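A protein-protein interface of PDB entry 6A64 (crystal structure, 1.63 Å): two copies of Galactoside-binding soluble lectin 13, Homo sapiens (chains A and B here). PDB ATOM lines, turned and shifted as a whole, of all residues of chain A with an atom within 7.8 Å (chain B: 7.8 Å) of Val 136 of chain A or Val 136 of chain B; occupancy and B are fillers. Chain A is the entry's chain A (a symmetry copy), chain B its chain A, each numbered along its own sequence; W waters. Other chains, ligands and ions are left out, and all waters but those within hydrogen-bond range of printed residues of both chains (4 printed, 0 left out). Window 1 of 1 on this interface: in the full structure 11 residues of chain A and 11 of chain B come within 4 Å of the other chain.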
ATOM      1  N   TYR A   7      17.546   8.484 -12.109  1.00  0.00           N
ATOM      2  CA  TYR A   7      18.139   9.767 -12.445  1.00  0.00           C
ATOM      3  C   TYR A   7      17.094  10.577 -13.199  1.00  0.00           C
ATOM      4  O   TYR A   7      16.665  10.175 -14.287  1.00  0.00           O
ATOM      5  CB  TYR A   7      19.396   9.561 -13.290  1.00  0.00           C
ATOM      6  CG  TYR A   7      20.077  10.828 -13.732  1.00  0.00           C
ATOM      7  CD1 TYR A   7      20.663  11.690 -12.810  1.00  0.00           C
ATOM      8  CD2 TYR A   7      20.149  11.154 -15.078  1.00  0.00           C
ATOM      9  CE1 TYR A   7      21.295  12.855 -13.232  1.00  0.00           C
ATOM     10  CE2 TYR A   7      20.771  12.307 -15.505  1.00  0.00           C
ATOM     11  CZ  TYR A   7      21.339  13.148 -14.584  1.00  0.00           C
ATOM     12  OH  TYR A   7      21.952  14.297 -15.041  1.00  0.00           O
ATOM     13  N   LEU A   9      16.430  14.000 -15.031  1.00  0.00           N
ATOM     14  CA  LEU A   9      17.144  15.120 -15.619  1.00  0.00           C
ATOM     15  C   LEU A   9      16.158  16.057 -16.291  1.00  0.00           C
ATOM     16  O   LEU A   9      15.507  15.655 -17.265  1.00  0.00           O
ATOM     17  CB  LEU A   9      18.174  14.618 -16.627  1.00  0.00           C
ATOM     18  CG  LEU A   9      18.894  15.684 -17.448  1.00  0.00           C
ATOM     19  CD1 LEU A   9      19.852  16.471 -16.550  1.00  0.00           C
ATOM     20  CD2 LEU A   9      19.623  15.041 -18.615  1.00  0.00           C
ATOM     21  N   PRO A  10      15.998  17.293 -15.820  1.00  0.00           N
ATOM     22  CA  PRO A  10      15.224  18.273 -16.590  1.00  0.00           C
ATOM     23  C   PRO A  10      15.894  18.520 -17.931  1.00  0.00           C
ATOM     24  O   PRO A  10      17.108  18.710 -18.015  1.00  0.00           O
ATOM     25  CB  PRO A  10      15.247  19.526 -15.703  1.00  0.00           C
ATOM     26  CG  PRO A  10      15.740  19.049 -14.355  1.00  0.00           C
ATOM     27  CD  PRO A  10      16.635  17.900 -14.639  1.00  0.00           C
ATOM     28  N   VAL A  11      15.097  18.505 -18.994  1.00  0.00           N
ATOM     29  CA  VAL A  11      15.626  18.633 -20.343  1.00  0.00           C
ATOM     30  C   VAL A  11      14.733  19.560 -21.147  1.00  0.00           C
ATOM     31  O   VAL A  11      13.572  19.805 -20.812  1.00  0.00           O
ATOM     32  CB  VAL A  11      15.739  17.286 -21.098  1.00  0.00           C
ATOM     33  CG1 VAL A  11      16.699  16.336 -20.407  1.00  0.00           C
ATOM     34  CG2 VAL A  11      14.356  16.645 -21.267  1.00  0.00           C
ATOM     35  N   SER A  12      15.313  20.095 -22.203  1.00  0.00           N
ATOM     36  CA  SER A  12      14.571  20.689 -23.299  1.00  0.00           C
ATOM     37  C   SER A  12      15.055  19.986 -24.554  1.00  0.00           C
ATOM     38  O   SER A  12      16.263  19.919 -24.799  1.00  0.00           O
ATOM     39  CB  SER A  12      14.797  22.207 -23.370  1.00  0.00           C
ATOM     40  OG  SER A  12      13.997  22.794 -24.380  1.00  0.00           O
ATOM     41  N   LEU A  13      14.130  19.415 -25.318  1.00  0.00           N
ATOM     42  CA  LEU A  13      14.479  18.677 -26.520  1.00  0.00           C
ATOM     43  C   LEU A  13      13.920  19.382 -27.743  1.00  0.00           C
ATOM     44  O   LEU A  13      12.823  19.944 -27.706  1.00  0.00           O
ATOM     45  CB  LEU A  13      13.948  17.239 -26.470  1.00  0.00           C
ATOM     46  CG  LEU A  13      14.518  16.361 -25.353  1.00  0.00           C
ATOM     47  CD1 LEU A  13      13.895  14.981 -25.445  1.00  0.00           C
ATOM     48  CD2 LEU A  13      16.032  16.267 -25.429  1.00  0.00           C
ATOM     49  N   SER A  14      14.688  19.358 -28.818  1.00  0.00           N
ATOM     50  CA  SER A  14      14.205  19.819 -30.105  1.00  0.00           C
ATOM     51  C   SER A  14      14.705  18.850 -31.159  1.00  0.00           C
ATOM     52  O   SER A  14      15.548  17.988 -30.894  1.00  0.00           O
ATOM     53  CB  SER A  14      14.671  21.246 -30.406  1.00  0.00           C
ATOM     54  OG  SER A  14      16.078  21.297 -30.531  1.00  0.00           O
ATOM     55  N   GLY A  16      16.970  17.447 -33.700  1.00  0.00           N
ATOM     56  CA  GLY A  16      18.410  17.556 -33.690  1.00  0.00           C
ATOM     57  C   GLY A  16      19.061  17.269 -32.350  1.00  0.00           C
ATOM     58  O   GLY A  16      20.283  17.085 -32.305  1.00  0.00           O
ATOM     59  N   SER A  17      18.288  17.217 -31.265  1.00  0.00           N
ATOM     60  CA  SER A  17      18.830  16.829 -29.964  1.00  0.00           C
ATOM     61  C   SER A  17      19.249  15.363 -29.955  1.00  0.00           C
ATOM     62  O   SER A  17      18.663  14.522 -30.641  1.00  0.00           O
ATOM     63  CB  SER A  17      17.801  17.048 -28.860  1.00  0.00           C
ATOM     64  OG  SER A  17      17.499  18.412 -28.686  1.00  0.00           O
ATOM     65  N   CYS A  18      20.267  15.057 -29.152  1.00  0.00           N
ATOM     66  CA  CYS A  18      20.675  13.677 -28.909  1.00  0.00           C
ATOM     67  C   CYS A  18      20.864  13.467 -27.417  1.00  0.00           C
ATOM     68  O   CYS A  18      21.566  14.250 -26.767  1.00  0.00           O
ATOM     69  CB  CYS A  18      21.973  13.327 -29.643  1.00  0.00           C
ATOM     70  SG  CYS A  18      22.315  11.549 -29.691  1.00  0.00           S
ATOM     71  N   VAL A  19      20.245  12.413 -26.879  1.00  0.00           N
ATOM     72  CA  VAL A  19      20.416  12.020 -25.483  1.00  0.00           C
ATOM     73  C   VAL A  19      21.337  10.811 -25.466  1.00  0.00           C
ATOM     74  O   VAL A  19      21.023   9.776 -26.063  1.00  0.00           O
ATOM     75  CB  VAL A  19      19.071  11.701 -24.810  1.00  0.00           C
ATOM     76  CG1 VAL A  19      19.287  11.210 -23.380  1.00  0.00           C
ATOM     77  CG2 VAL A  19      18.151  12.916 -24.831  1.00  0.00           C
ATOM     78  N   ILE A  20      22.481  10.939 -24.801  1.00  0.00           N
ATOM     79  CA  ILE A  20      23.494   9.888 -24.770  1.00  0.00           C
ATOM     80  C   ILE A  20      23.646   9.411 -23.334  1.00  0.00           C
ATOM     81  O   ILE A  20      24.039  10.186 -22.453  1.00  0.00           O
ATOM     82  CB  ILE A  20      24.838  10.375 -25.339  1.00  0.00           C
ATOM     83  CG1 ILE A  20      24.623  11.026 -26.703  1.00  0.00           C
ATOM     84  CG2 ILE A  20      25.831   9.222 -25.435  1.00  0.00           C
ATOM     85  CD1 ILE A  20      24.908  12.516 -26.717  1.00  0.00           C
ATOM     86  N   ILE A  21      23.344   8.135 -23.104  1.00  0.00           N
ATOM     87  CA  ILE A  21      23.336   7.539 -21.769  1.00  0.00           C
ATOM     88  C   ILE A  21      24.388   6.441 -21.741  1.00  0.00           C
ATOM     89  O   ILE A  21      24.334   5.507 -22.547  1.00  0.00           O
ATOM     90  CB  ILE A  21      21.954   6.972 -21.410  1.00  0.00           C
ATOM     91  CG1 ILE A  21      20.918   8.091 -21.282  1.00  0.00           C
ATOM     92  CG2 ILE A  21      22.016   6.156 -20.144  1.00  0.00           C
ATOM     93  CD1 ILE A  21      19.499   7.617 -21.610  1.00  0.00           C
ATOM     94  N   ILE A  92      19.710   8.274 -28.036  1.00  0.00           N
ATOM     95  CA  ILE A  92      18.370   8.557 -28.527  1.00  0.00           C
ATOM     96  C   ILE A  92      18.428   9.888 -29.264  1.00  0.00           C
ATOM     97  O   ILE A  92      18.635  10.946 -28.652  1.00  0.00           O
ATOM     98  CB  ILE A  92      17.330   8.578 -27.403  1.00  0.00           C
ATOM     99  CG1 ILE A  92      17.368   7.250 -26.644  1.00  0.00           C
ATOM    100  CG2 ILE A  92      15.947   8.809 -27.993  1.00  0.00           C
ATOM    101  CD1 ILE A  92      16.646   7.284 -25.327  1.00  0.00           C
ATOM    102  N   VAL A  94      16.663  12.752 -31.624  1.00  0.00           N
ATOM    103  CA  VAL A  94      15.352  13.326 -31.902  1.00  0.00           C
ATOM    104  C   VAL A  94      15.351  13.791 -33.353  1.00  0.00           C
ATOM    105  O   VAL A  94      15.915  14.834 -33.680  1.00  0.00           O
ATOM    106  CB  VAL A  94      15.028  14.478 -30.950  1.00  0.00           C
ATOM    107  CG1 VAL A  94      13.602  14.951 -31.172  1.00  0.00           C
ATOM    108  CG2 VAL A  94      15.221  14.046 -29.528  1.00  0.00           C
ATOM    109  N   VAL A 123      13.885  13.659 -18.514  1.00  0.00           N
ATOM    110  CA  VAL A 123      14.266  12.318 -18.929  1.00  0.00           C
ATOM    111  C   VAL A 123      14.615  11.557 -17.669  1.00  0.00           C
ATOM    112  O   VAL A 123      15.452  12.016 -16.883  1.00  0.00           O
ATOM    113  CB  VAL A 123      15.443  12.334 -19.912  1.00  0.00           C
ATOM    114  CG1 VAL A 123      15.965  10.937 -20.141  1.00  0.00           C
ATOM    115  CG2 VAL A 123      15.012  12.954 -21.235  1.00  0.00           C
ATOM    116  N   VAL A 134      25.261  11.113 -18.509  1.00  0.00           N
ATOM    117  CA  VAL A 134      24.133  11.432 -19.379  1.00  0.00           C
ATOM    118  C   VAL A 134      24.429  12.781 -20.025  1.00  0.00           C
ATOM    119  O   VAL A 134      24.714  13.758 -19.322  1.00  0.00           O
ATOM    120  CB  VAL A 134      22.794  11.475 -18.625  1.00  0.00           C
ATOM    121  CG1 VAL A 134      21.655  11.751 -19.596  1.00  0.00           C
ATOM    122  CG2 VAL A 134      22.538  10.150 -17.871  1.00  0.00           C
ATOM    123  N   CYS A 135      24.386  12.831 -21.348  1.00  0.00           N
ATOM    124  CA  CYS A 135      24.642  14.057 -22.101  1.00  0.00           C
ATOM    125  C   CYS A 135      23.457  14.358 -23.004  1.00  0.00           C
ATOM    126  O   CYS A 135      22.844  13.442 -23.555  1.00  0.00           O
ATOM    127  CB  CYS A 135      25.903  13.941 -22.962  1.00  0.00           C
ATOM    128  SG  CYS A 135      27.453  13.795 -22.083  1.00  0.00           S
ATOM    129  N   VAL A 136      23.149  15.643 -23.169  1.00  0.00           N
ATOM    130  CA  VAL A 136      22.168  16.111 -24.141  1.00  0.00           C
ATOM    131  C   VAL A 136      22.888  17.066 -25.085  1.00  0.00           C
ATOM    132  O   VAL A 136      23.405  18.100 -24.649  1.00  0.00           O
ATOM    133  CB  VAL A 136      20.971  16.797 -23.469  1.00  0.00           C
ATOM    134  CG1 VAL A 136      19.983  17.275 -24.521  1.00  0.00           C
ATOM    135  CG2 VAL A 136      20.289  15.820 -22.502  1.00  0.00           C
ATOM    136  N   CYS A 137      22.934  16.711 -26.365  1.00  0.00           N
ATOM    137  CA  CYS A 137      23.722  17.447 -27.346  1.00  0.00           C
ATOM    138  C   CYS A 137      22.838  18.001 -28.450  1.00  0.00           C
ATOM    139  O   CYS A 137      21.781  17.446 -28.760  1.00  0.00           O
ATOM    140  CB  CYS A 137      24.797  16.556 -27.987  1.00  0.00           C
ATOM    141  SG  CYS A 137      26.169  16.119 -26.889  1.00  0.00           S
ATOM    142  N   ASN A 138      23.281  19.116 -29.027  1.00  0.00           N
ATOM    143  CA  ASN A 138      22.666  19.678 -30.226  1.00  0.00           C
ATOM    144  C   ASN A 138      23.755  20.124 -31.192  1.00  0.00           C
ATOM    145  O   ASN A 138      24.918  20.237 -30.807  1.00  0.00           O
ATOM    146  CB  ASN A 138      21.758  20.858 -29.884  1.00  0.00           C
ATOM    147  CG  ASN A 138      20.599  20.462 -28.994  1.00  0.00           C
ATOM    148  OD1 ASN A 138      19.522  20.114 -29.479  1.00  0.00           O
ATOM    149  ND2 ASN A 138      20.813  20.510 -27.686  1.00  0.00           N
ATOM    150  N   TYR B   7      22.491  31.461 -30.345  1.00  0.00           N
ATOM    151  CA  TYR B   7      21.917  30.168 -30.017  1.00  0.00           C
ATOM    152  C   TYR B   7      21.422  30.231 -28.579  1.00  0.00           C
ATOM    153  O   TYR B   7      22.222  30.423 -27.656  1.00  0.00           O
ATOM    154  CB  TYR B   7      22.962  29.067 -30.194  1.00  0.00           C
ATOM    155  CG  TYR B   7      22.490  27.681 -29.844  1.00  0.00           C
ATOM    156  CD1 TYR B   7      21.493  27.053 -30.584  1.00  0.00           C
ATOM    157  CD2 TYR B   7      23.056  26.994 -28.782  1.00  0.00           C
ATOM    158  CE1 TYR B   7      21.068  25.770 -30.254  1.00  0.00           C
ATOM    159  CE2 TYR B   7      22.640  25.723 -28.446  1.00  0.00           C
ATOM    160  CZ  TYR B   7      21.653  25.119 -29.182  1.00  0.00           C
ATOM    161  OH  TYR B   7      21.257  23.849 -28.820  1.00  0.00           O
ATOM    162  N   LEU B   9      19.724  28.149 -25.700  1.00  0.00           N
ATOM    163  CA  LEU B   9      19.457  26.775 -25.309  1.00  0.00           C
ATOM    164  C   LEU B   9      18.837  26.749 -23.925  1.00  0.00           C
ATOM    165  O   LEU B   9      19.501  27.144 -22.956  1.00  0.00           O
ATOM    166  CB  LEU B   9      20.748  25.960 -25.331  1.00  0.00           C
ATOM    167  CG  LEU B   9      20.658  24.536 -24.790  1.00  0.00           C
ATOM    168  CD1 LEU B   9      19.849  23.665 -25.754  1.00  0.00           C
ATOM    169  CD2 LEU B   9      22.052  23.974 -24.565  1.00  0.00           C
ATOM    170  N   PRO B  10      17.588  26.313 -23.770  1.00  0.00           N
ATOM    171  CA  PRO B  10      17.061  26.072 -22.423  1.00  0.00           C
ATOM    172  C   PRO B  10      17.872  24.984 -21.739  1.00  0.00           C
ATOM    173  O   PRO B  10      18.164  23.939 -22.323  1.00  0.00           O
ATOM    174  CB  PRO B  10      15.614  25.627 -22.678  1.00  0.00           C
ATOM    175  CG  PRO B  10      15.338  25.980 -24.122  1.00  0.00           C
ATOM    176  CD  PRO B  10      16.646  25.879 -24.816  1.00  0.00           C
ATOM    177  N   VAL B  11      18.252  25.236 -20.491  1.00  0.00           N
ATOM    178  CA  VAL B  11      19.112  24.319 -19.759  1.00  0.00           C
ATOM    179  C   VAL B  11      18.607  24.186 -18.334  1.00  0.00           C
ATOM    180  O   VAL B  11      17.860  25.023 -17.823  1.00  0.00           O
ATOM    181  CB  VAL B  11      20.596  24.760 -19.712  1.00  0.00           C
ATOM    182  CG1 VAL B  11      21.206  24.819 -21.100  1.00  0.00           C
ATOM    183  CG2 VAL B  11      20.736  26.106 -18.991  1.00  0.00           C
ATOM    184  N   SER B  12      19.008  23.094 -17.713  1.00  0.00           N
ATOM    185  CA  SER B  12      18.969  22.943 -16.271  1.00  0.00           C
ATOM    186  C   SER B  12      20.381  22.570 -15.858  1.00  0.00           C
ATOM    187  O   SER B  12      20.957  21.624 -16.404  1.00  0.00           O
ATOM    188  CB  SER B  12      17.948  21.876 -15.847  1.00  0.00           C
ATOM    189  OG  SER B  12      17.846  21.801 -14.437  1.00  0.00           O
ATOM    190  N   LEU B  13      20.962  23.336 -14.941  1.00  0.00           N
ATOM    191  CA  LEU B  13      22.326  23.102 -14.500  1.00  0.00           C
ATOM    192  C   LEU B  13      22.337  22.708 -13.033  1.00  0.00           C
ATOM    193  O   LEU B  13      21.548  23.217 -12.233  1.00  0.00           O
ATOM    194  CB  LEU B  13      23.203  24.344 -14.702  1.00  0.00           C
ATOM    195  CG  LEU B  13      23.386  24.794 -16.154  1.00  0.00           C
ATOM    196  CD1 LEU B  13      24.275  26.024 -16.180  1.00  0.00           C
ATOM    197  CD2 LEU B  13      23.981  23.692 -17.014  1.00  0.00           C
ATOM    198  N   SER B  14      23.226  21.792 -12.694  1.00  0.00           N
ATOM    199  CA  SER B  14      23.481  21.460 -11.305  1.00  0.00           C
ATOM    200  C   SER B  14      24.979  21.295 -11.138  1.00  0.00           C
ATOM    201  O   SER B  14      25.735  21.250 -12.113  1.00  0.00           O
ATOM    202  CB  SER B  14      22.738  20.190 -10.881  1.00  0.00           C
ATOM    203  OG  SER B  14      23.218  19.068 -11.594  1.00  0.00           O
ATOM    204  N   GLY B  16      28.229  19.568 -11.045  1.00  0.00           N
ATOM    205  CA  GLY B  16      28.598  18.433 -11.858  1.00  0.00           C
ATOM    206  C   GLY B  16      28.235  18.557 -13.326  1.00  0.00           C
ATOM    207  O   GLY B  16      28.734  17.765 -14.134  1.00  0.00           O
ATOM    208  N   SER B  17      27.396  19.524 -13.694  1.00  0.00           N
ATOM    209  CA  SER B  17      27.097  19.774 -15.103  1.00  0.00           C
ATOM    210  C   SER B  17      28.320  20.307 -15.841  1.00  0.00           C
ATOM    211  O   SER B  17      29.163  21.002 -15.270  1.00  0.00           O
ATOM    212  CB  SER B  17      25.962  20.782 -15.248  1.00  0.00           C
ATOM    213  OG  SER B  17      24.746  20.280 -14.747  1.00  0.00           O
ATOM    214  N   CYS B  18      28.401  19.990 -17.133  1.00  0.00           N
ATOM    215  CA  CYS B  18      29.420  20.560 -18.009  1.00  0.00           C
ATOM    216  C   CYS B  18      28.764  21.035 -19.294  1.00  0.00           C
ATOM    217  O   CYS B  18      28.022  20.276 -19.925  1.00  0.00           O
ATOM    218  CB  CYS B  18      30.520  19.549 -18.340  1.00  0.00           C
ATOM    219  SG  CYS B  18      31.986  20.301 -19.094  1.00  0.00           S
ATOM    220  N   VAL B  19      29.042  22.283 -19.680  1.00  0.00           N
ATOM    221  CA  VAL B  19      28.574  22.844 -20.944  1.00  0.00           C
ATOM    222  C   VAL B  19      29.758  22.859 -21.896  1.00  0.00           C
ATOM    223  O   VAL B  19      30.781  23.491 -21.614  1.00  0.00           O
ATOM    224  CB  VAL B  19      27.993  24.256 -20.762  1.00  0.00           C
ATOM    225  CG1 VAL B  19      27.592  24.852 -22.111  1.00  0.00           C
ATOM    226  CG2 VAL B  19      26.806  24.237 -19.806  1.00  0.00           C
ATOM    227  N   ILE B  20      29.636  22.150 -23.015  1.00  0.00           N
ATOM    228  CA  ILE B  20      30.725  22.009 -23.978  1.00  0.00           C
ATOM    229  C   ILE B  20      30.289  22.647 -25.288  1.00  0.00           C
ATOM    230  O   ILE B  20      29.320  22.199 -25.914  1.00  0.00           O
ATOM    231  CB  ILE B  20      31.119  20.536 -24.181  1.00  0.00           C
ATOM    232  CG1 ILE B  20      31.361  19.869 -22.829  1.00  0.00           C
ATOM    233  CG2 ILE B  20      32.351  20.426 -25.071  1.00  0.00           C
ATOM    234  CD1 ILE B  20      30.346  18.793 -22.491  1.00  0.00           C
ATOM    235  N   ILE B  21      31.013  23.684 -25.706  1.00  0.00           N
ATOM    236  CA  ILE B  21      30.676  24.475 -26.887  1.00  0.00           C
ATOM    237  C   ILE B  21      31.812  24.331 -27.887  1.00  0.00           C
ATOM    238  O   ILE B  21      32.965  24.642 -27.568  1.00  0.00           O
ATOM    239  CB  ILE B  21      30.452  25.953 -26.533  1.00  0.00           C
ATOM    240  CG1 ILE B  21      29.213  26.126 -25.652  1.00  0.00           C
ATOM    241  CG2 ILE B  21      30.341  26.797 -27.778  1.00  0.00           C
ATOM    242  CD1 ILE B  21      29.310  27.351 -24.737  1.00  0.00           C
ATOM    243  N   ILE B  92      32.641  24.683 -19.883  1.00  0.00           N
ATOM    244  CA  ILE B  92      32.292  25.358 -18.643  1.00  0.00           C
ATOM    245  C   ILE B  92      31.747  24.304 -17.689  1.00  0.00           C
ATOM    246  O   ILE B  92      30.664  23.743 -17.912  1.00  0.00           O
ATOM    247  CB  ILE B  92      31.291  26.496 -18.860  1.00  0.00           C
ATOM    248  CG1 ILE B  92      31.851  27.485 -19.885  1.00  0.00           C
ATOM    249  CG2 ILE B  92      31.024  27.200 -17.539  1.00  0.00           C
ATOM    250  CD1 ILE B  92      30.827  28.441 -20.427  1.00  0.00           C
ATOM    251  N   VAL B  94      30.427  23.190 -13.960  1.00  0.00           N
ATOM    252  CA  VAL B  94      29.746  23.748 -12.798  1.00  0.00           C
ATOM    253  C   VAL B  94      30.246  22.999 -11.568  1.00  0.00           C
ATOM    254  O   VAL B  94      29.836  21.868 -11.310  1.00  0.00           O
ATOM    255  CB  VAL B  94      28.226  23.641 -12.931  1.00  0.00           C
ATOM    256  CG1 VAL B  94      27.551  24.362 -11.777  1.00  0.00           C
ATOM    257  CG2 VAL B  94      27.779  24.218 -14.241  1.00  0.00           C
ATOM    258  N   VAL B 123      21.209  29.091 -21.745  1.00  0.00           N
ATOM    259  CA  VAL B 123      22.574  29.442 -22.105  1.00  0.00           C
ATOM    260  C   VAL B 123      22.516  30.037 -23.495  1.00  0.00           C
ATOM    261  O   VAL B 123      21.979  29.408 -24.415  1.00  0.00           O
ATOM    262  CB  VAL B 123      23.509  28.227 -22.060  1.00  0.00           C
ATOM    263  CG1 VAL B 123      24.852  28.566 -22.658  1.00  0.00           C
ATOM    264  CG2 VAL B 123      23.683  27.753 -20.622  1.00  0.00           C
ATOM    265  N   VAL B 134      26.710  22.059 -29.241  1.00  0.00           N
ATOM    266  CA  VAL B 134      26.623  22.431 -27.832  1.00  0.00           C
ATOM    267  C   VAL B 134      26.086  21.218 -27.079  1.00  0.00           C
ATOM    268  O   VAL B 134      25.035  20.675 -27.442  1.00  0.00           O
ATOM    269  CB  VAL B 134      25.726  23.656 -27.593  1.00  0.00           C
ATOM    270  CG1 VAL B 134      25.727  24.026 -26.117  1.00  0.00           C
ATOM    271  CG2 VAL B 134      26.194  24.860 -28.442  1.00  0.00           C
ATOM    272  N   CYS B 135      26.808  20.782 -26.058  1.00  0.00           N
ATOM    273  CA  CYS B 135      26.414  19.635 -25.243  1.00  0.00           C
ATOM    274  C   CYS B 135      26.341  20.048 -23.782  1.00  0.00           C
ATOM    275  O   CYS B 135      27.153  20.851 -23.319  1.00  0.00           O
ATOM    276  CB  CYS B 135      27.402  18.475 -25.381  1.00  0.00           C
ATOM    277  SG  CYS B 135      27.488  17.692 -26.985  1.00  0.00           S
ATOM    278  N   VAL B 136      25.380  19.483 -23.054  1.00  0.00           N
ATOM    279  CA  VAL B 136      25.287  19.624 -21.605  1.00  0.00           C
ATOM    280  C   VAL B 136      25.353  18.223 -21.010  1.00  0.00           C
ATOM    281  O   VAL B 136      24.490  17.386 -21.293  1.00  0.00           O
ATOM    282  CB  VAL B 136      24.003  20.346 -21.176  1.00  0.00           C
ATOM    283  CG1 VAL B 136      23.948  20.460 -19.661  1.00  0.00           C
ATOM    284  CG2 VAL B 136      23.952  21.740 -21.818  1.00  0.00           C
ATOM    285  N   CYS B 137      26.381  17.969 -20.207  1.00  0.00           N
ATOM    286  CA  CYS B 137      26.654  16.631 -19.696  1.00  0.00           C
ATOM    287  C   CYS B 137      26.605  16.606 -18.178  1.00  0.00           C
ATOM    288  O   CYS B 137      26.867  17.613 -17.516  1.00  0.00           O
ATOM    289  CB  CYS B 137      28.035  16.129 -20.146  1.00  0.00           C
ATOM    290  SG  CYS B 137      28.154  15.719 -21.905  1.00  0.00           S
ATOM    291  N   ASN B 138      26.250  15.442 -17.640  1.00  0.00           N
ATOM    292  CA  ASN B 138      26.336  15.179 -16.206  1.00  0.00           C
ATOM    293  C   ASN B 138      26.912  13.789 -15.980  1.00  0.00           C
ATOM    294  O   ASN B 138      26.971  12.983 -16.907  1.00  0.00           O
ATOM    295  CB  ASN B 138      24.967  15.291 -15.538  1.00  0.00           C
ATOM    296  CG  ASN B 138      24.375  16.682 -15.651  1.00  0.00           C
ATOM    297  OD1 ASN B 138      24.578  17.526 -14.778  1.00  0.00           O
ATOM    298  ND2 ASN B 138      23.643  16.927 -16.729  1.00  0.00           N
HETATM  299  O   HOH W   1      21.622  16.282 -13.463  1.00  0.00           O
HETATM  300  O   HOH W   2      22.823  14.892 -17.924  1.00  0.00           O
HETATM  301  O   HOH W   3      22.773  21.899 -26.996  1.00  0.00           O
HETATM  302  O   HOH W   4      18.747  23.475 -29.138  1.00  0.00           O
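The backbone NH of Asn 138 of chain A sits at hydrogen-bond distance from the backbone carbonyl oxygen of Val 134 of chain B (2.8 Å).
O of Val 136 of chain A sits at hydrogen-bond distance from N of Val 136 of chain B.
The side-chain sulfur (SG) of Cys 137 of chain A is disulfide-bonded to the side-chain sulfur (SG) of Cys 135 of chain B (2.1 Å).
O of Val 134 of chain A sits at hydrogen-bond distance from N of Asn 138 of chain B, at 2.8 Å.
SG of Cys 135 of chain A is disulfide-bonded to SG of Cys 137 of chain B, at 2.1 Å.
O of Leu 9 of chain B lies within hydrogen-bond range of N of Val 123 of chain B (2.9 Å).
The backbone carbonyl oxygen (O) of Cys 18 of chain A sits at hydrogen-bond distance from the backbone NH (N) of Cys 137 of chain A (2.8 Å).
The side-chain hydroxyl (OG) of Ser 17 of chain A is in hydrogen-bond range of the side-chain amide oxygen (OD1) of Asn 138 of chain A.
OH of Tyr 7 of chain A touches CB of Asn 138 of chain B (3.2 Å).
Leu 9 of chain A touches Asn 138 of chain B (CD1 to ND2, 3.8 Å).
CG of Pro 10 of chain A touches OG of Ser 12 of chain B, 3.5 Å away.
Ser 12 of chain A touches Pro 10 of chain B.
Cys 137 of chain B touches Val 134 of chain A (CA to O, 3.5 Å).
Val 136 of chain A touches Cys 135 of chain B (O to CA, 3.4 Å).
Cys 137 of chain A touches Val 134 of chain B (CA to O, 3.5 Å).
Val 136 of chain A touches just these residues of chain B: Cys 135 and Val 136.
Val 136 of chain B touches two residues of chain A.
Of the printed residues of chain B, Asn 138 of chain A touches Tyr 7, Leu 9 and Val 134.
Of the printed residues of chain A, Ser 12 of chain B touches Pro 10 (3.5 Å).
Printed residues of chain A within 4 Å of Leu 9 of chain B: Asn 138.
Of the printed residues of chain A, Cys 137 of chain B touches Val 134 and Cys 135.
Ile 20 of chain B touches none of the printed residues of chain A.
The nearest residue of chain B that does not touch Val 136 of chain A is Val 134 of chain B (4.1 Å).
The nearest printed residue of chain B that does not touch Tyr 7 of chain A is Ser 14 of chain B (6.0 Å).
Of the 21 printed residues of chain B, 9 touch a printed residue of chain A.
Hydrophobic or aromatic side chains of chain B within 4 Å of the printed part of chain A: Tyr 7, Leu 9 and Pro 10.
Of the 21 printed residues of chain A, 9 touch a printed residue of chain B.
Printed residues of chain A that touch a printed residue of chain B: Tyr 7, Leu 9, Pro 10, Ser 12, Val 134, Cys 135, Val 136, Cys 137 and Asn 138.
Along chain A the printed residues that touch a printed residue of chain B span positions 7 to 138.
Among the printed residues, no Asp or Glu carboxylate lies within 4 Å of a Lys or Arg side-chain nitrogen of the other chain.
Tyr 7 of chain A touches Asn 138 of chain B, and with the chains exchanged Asn 138 of chain A touches Tyr 7 of chain B.
Leu 9 of chain A touches Asn 138 of chain B, and with the chains exchanged Asn 138 of chain A touches Leu 9 of chain B.
Pro 10 of chain A touches Ser 12 of chain B, and with the chains exchanged Ser 12 of chain A touches Pro 10 of chain B.
Val 136 of chain A touches its own counterpart, Val 136 of chain B.
Water W3 lies within hydrogen-bond range of ND2 of Asn 138 of chain A (2.5 Å), O of Val 134 of chain B (2.6 Å) and OH of Tyr 7 of chain B (3.1 Å).
Water W2 lies within hydrogen-bond range of the side-chain amide nitrogen of Asn 138 of chain B (2.5 Å), the backbone carbonyl oxygen of Val 134 of chain A (2.6 Å) and the side-chain hydroxyl of Tyr 7 of chain A (3.1 Å).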
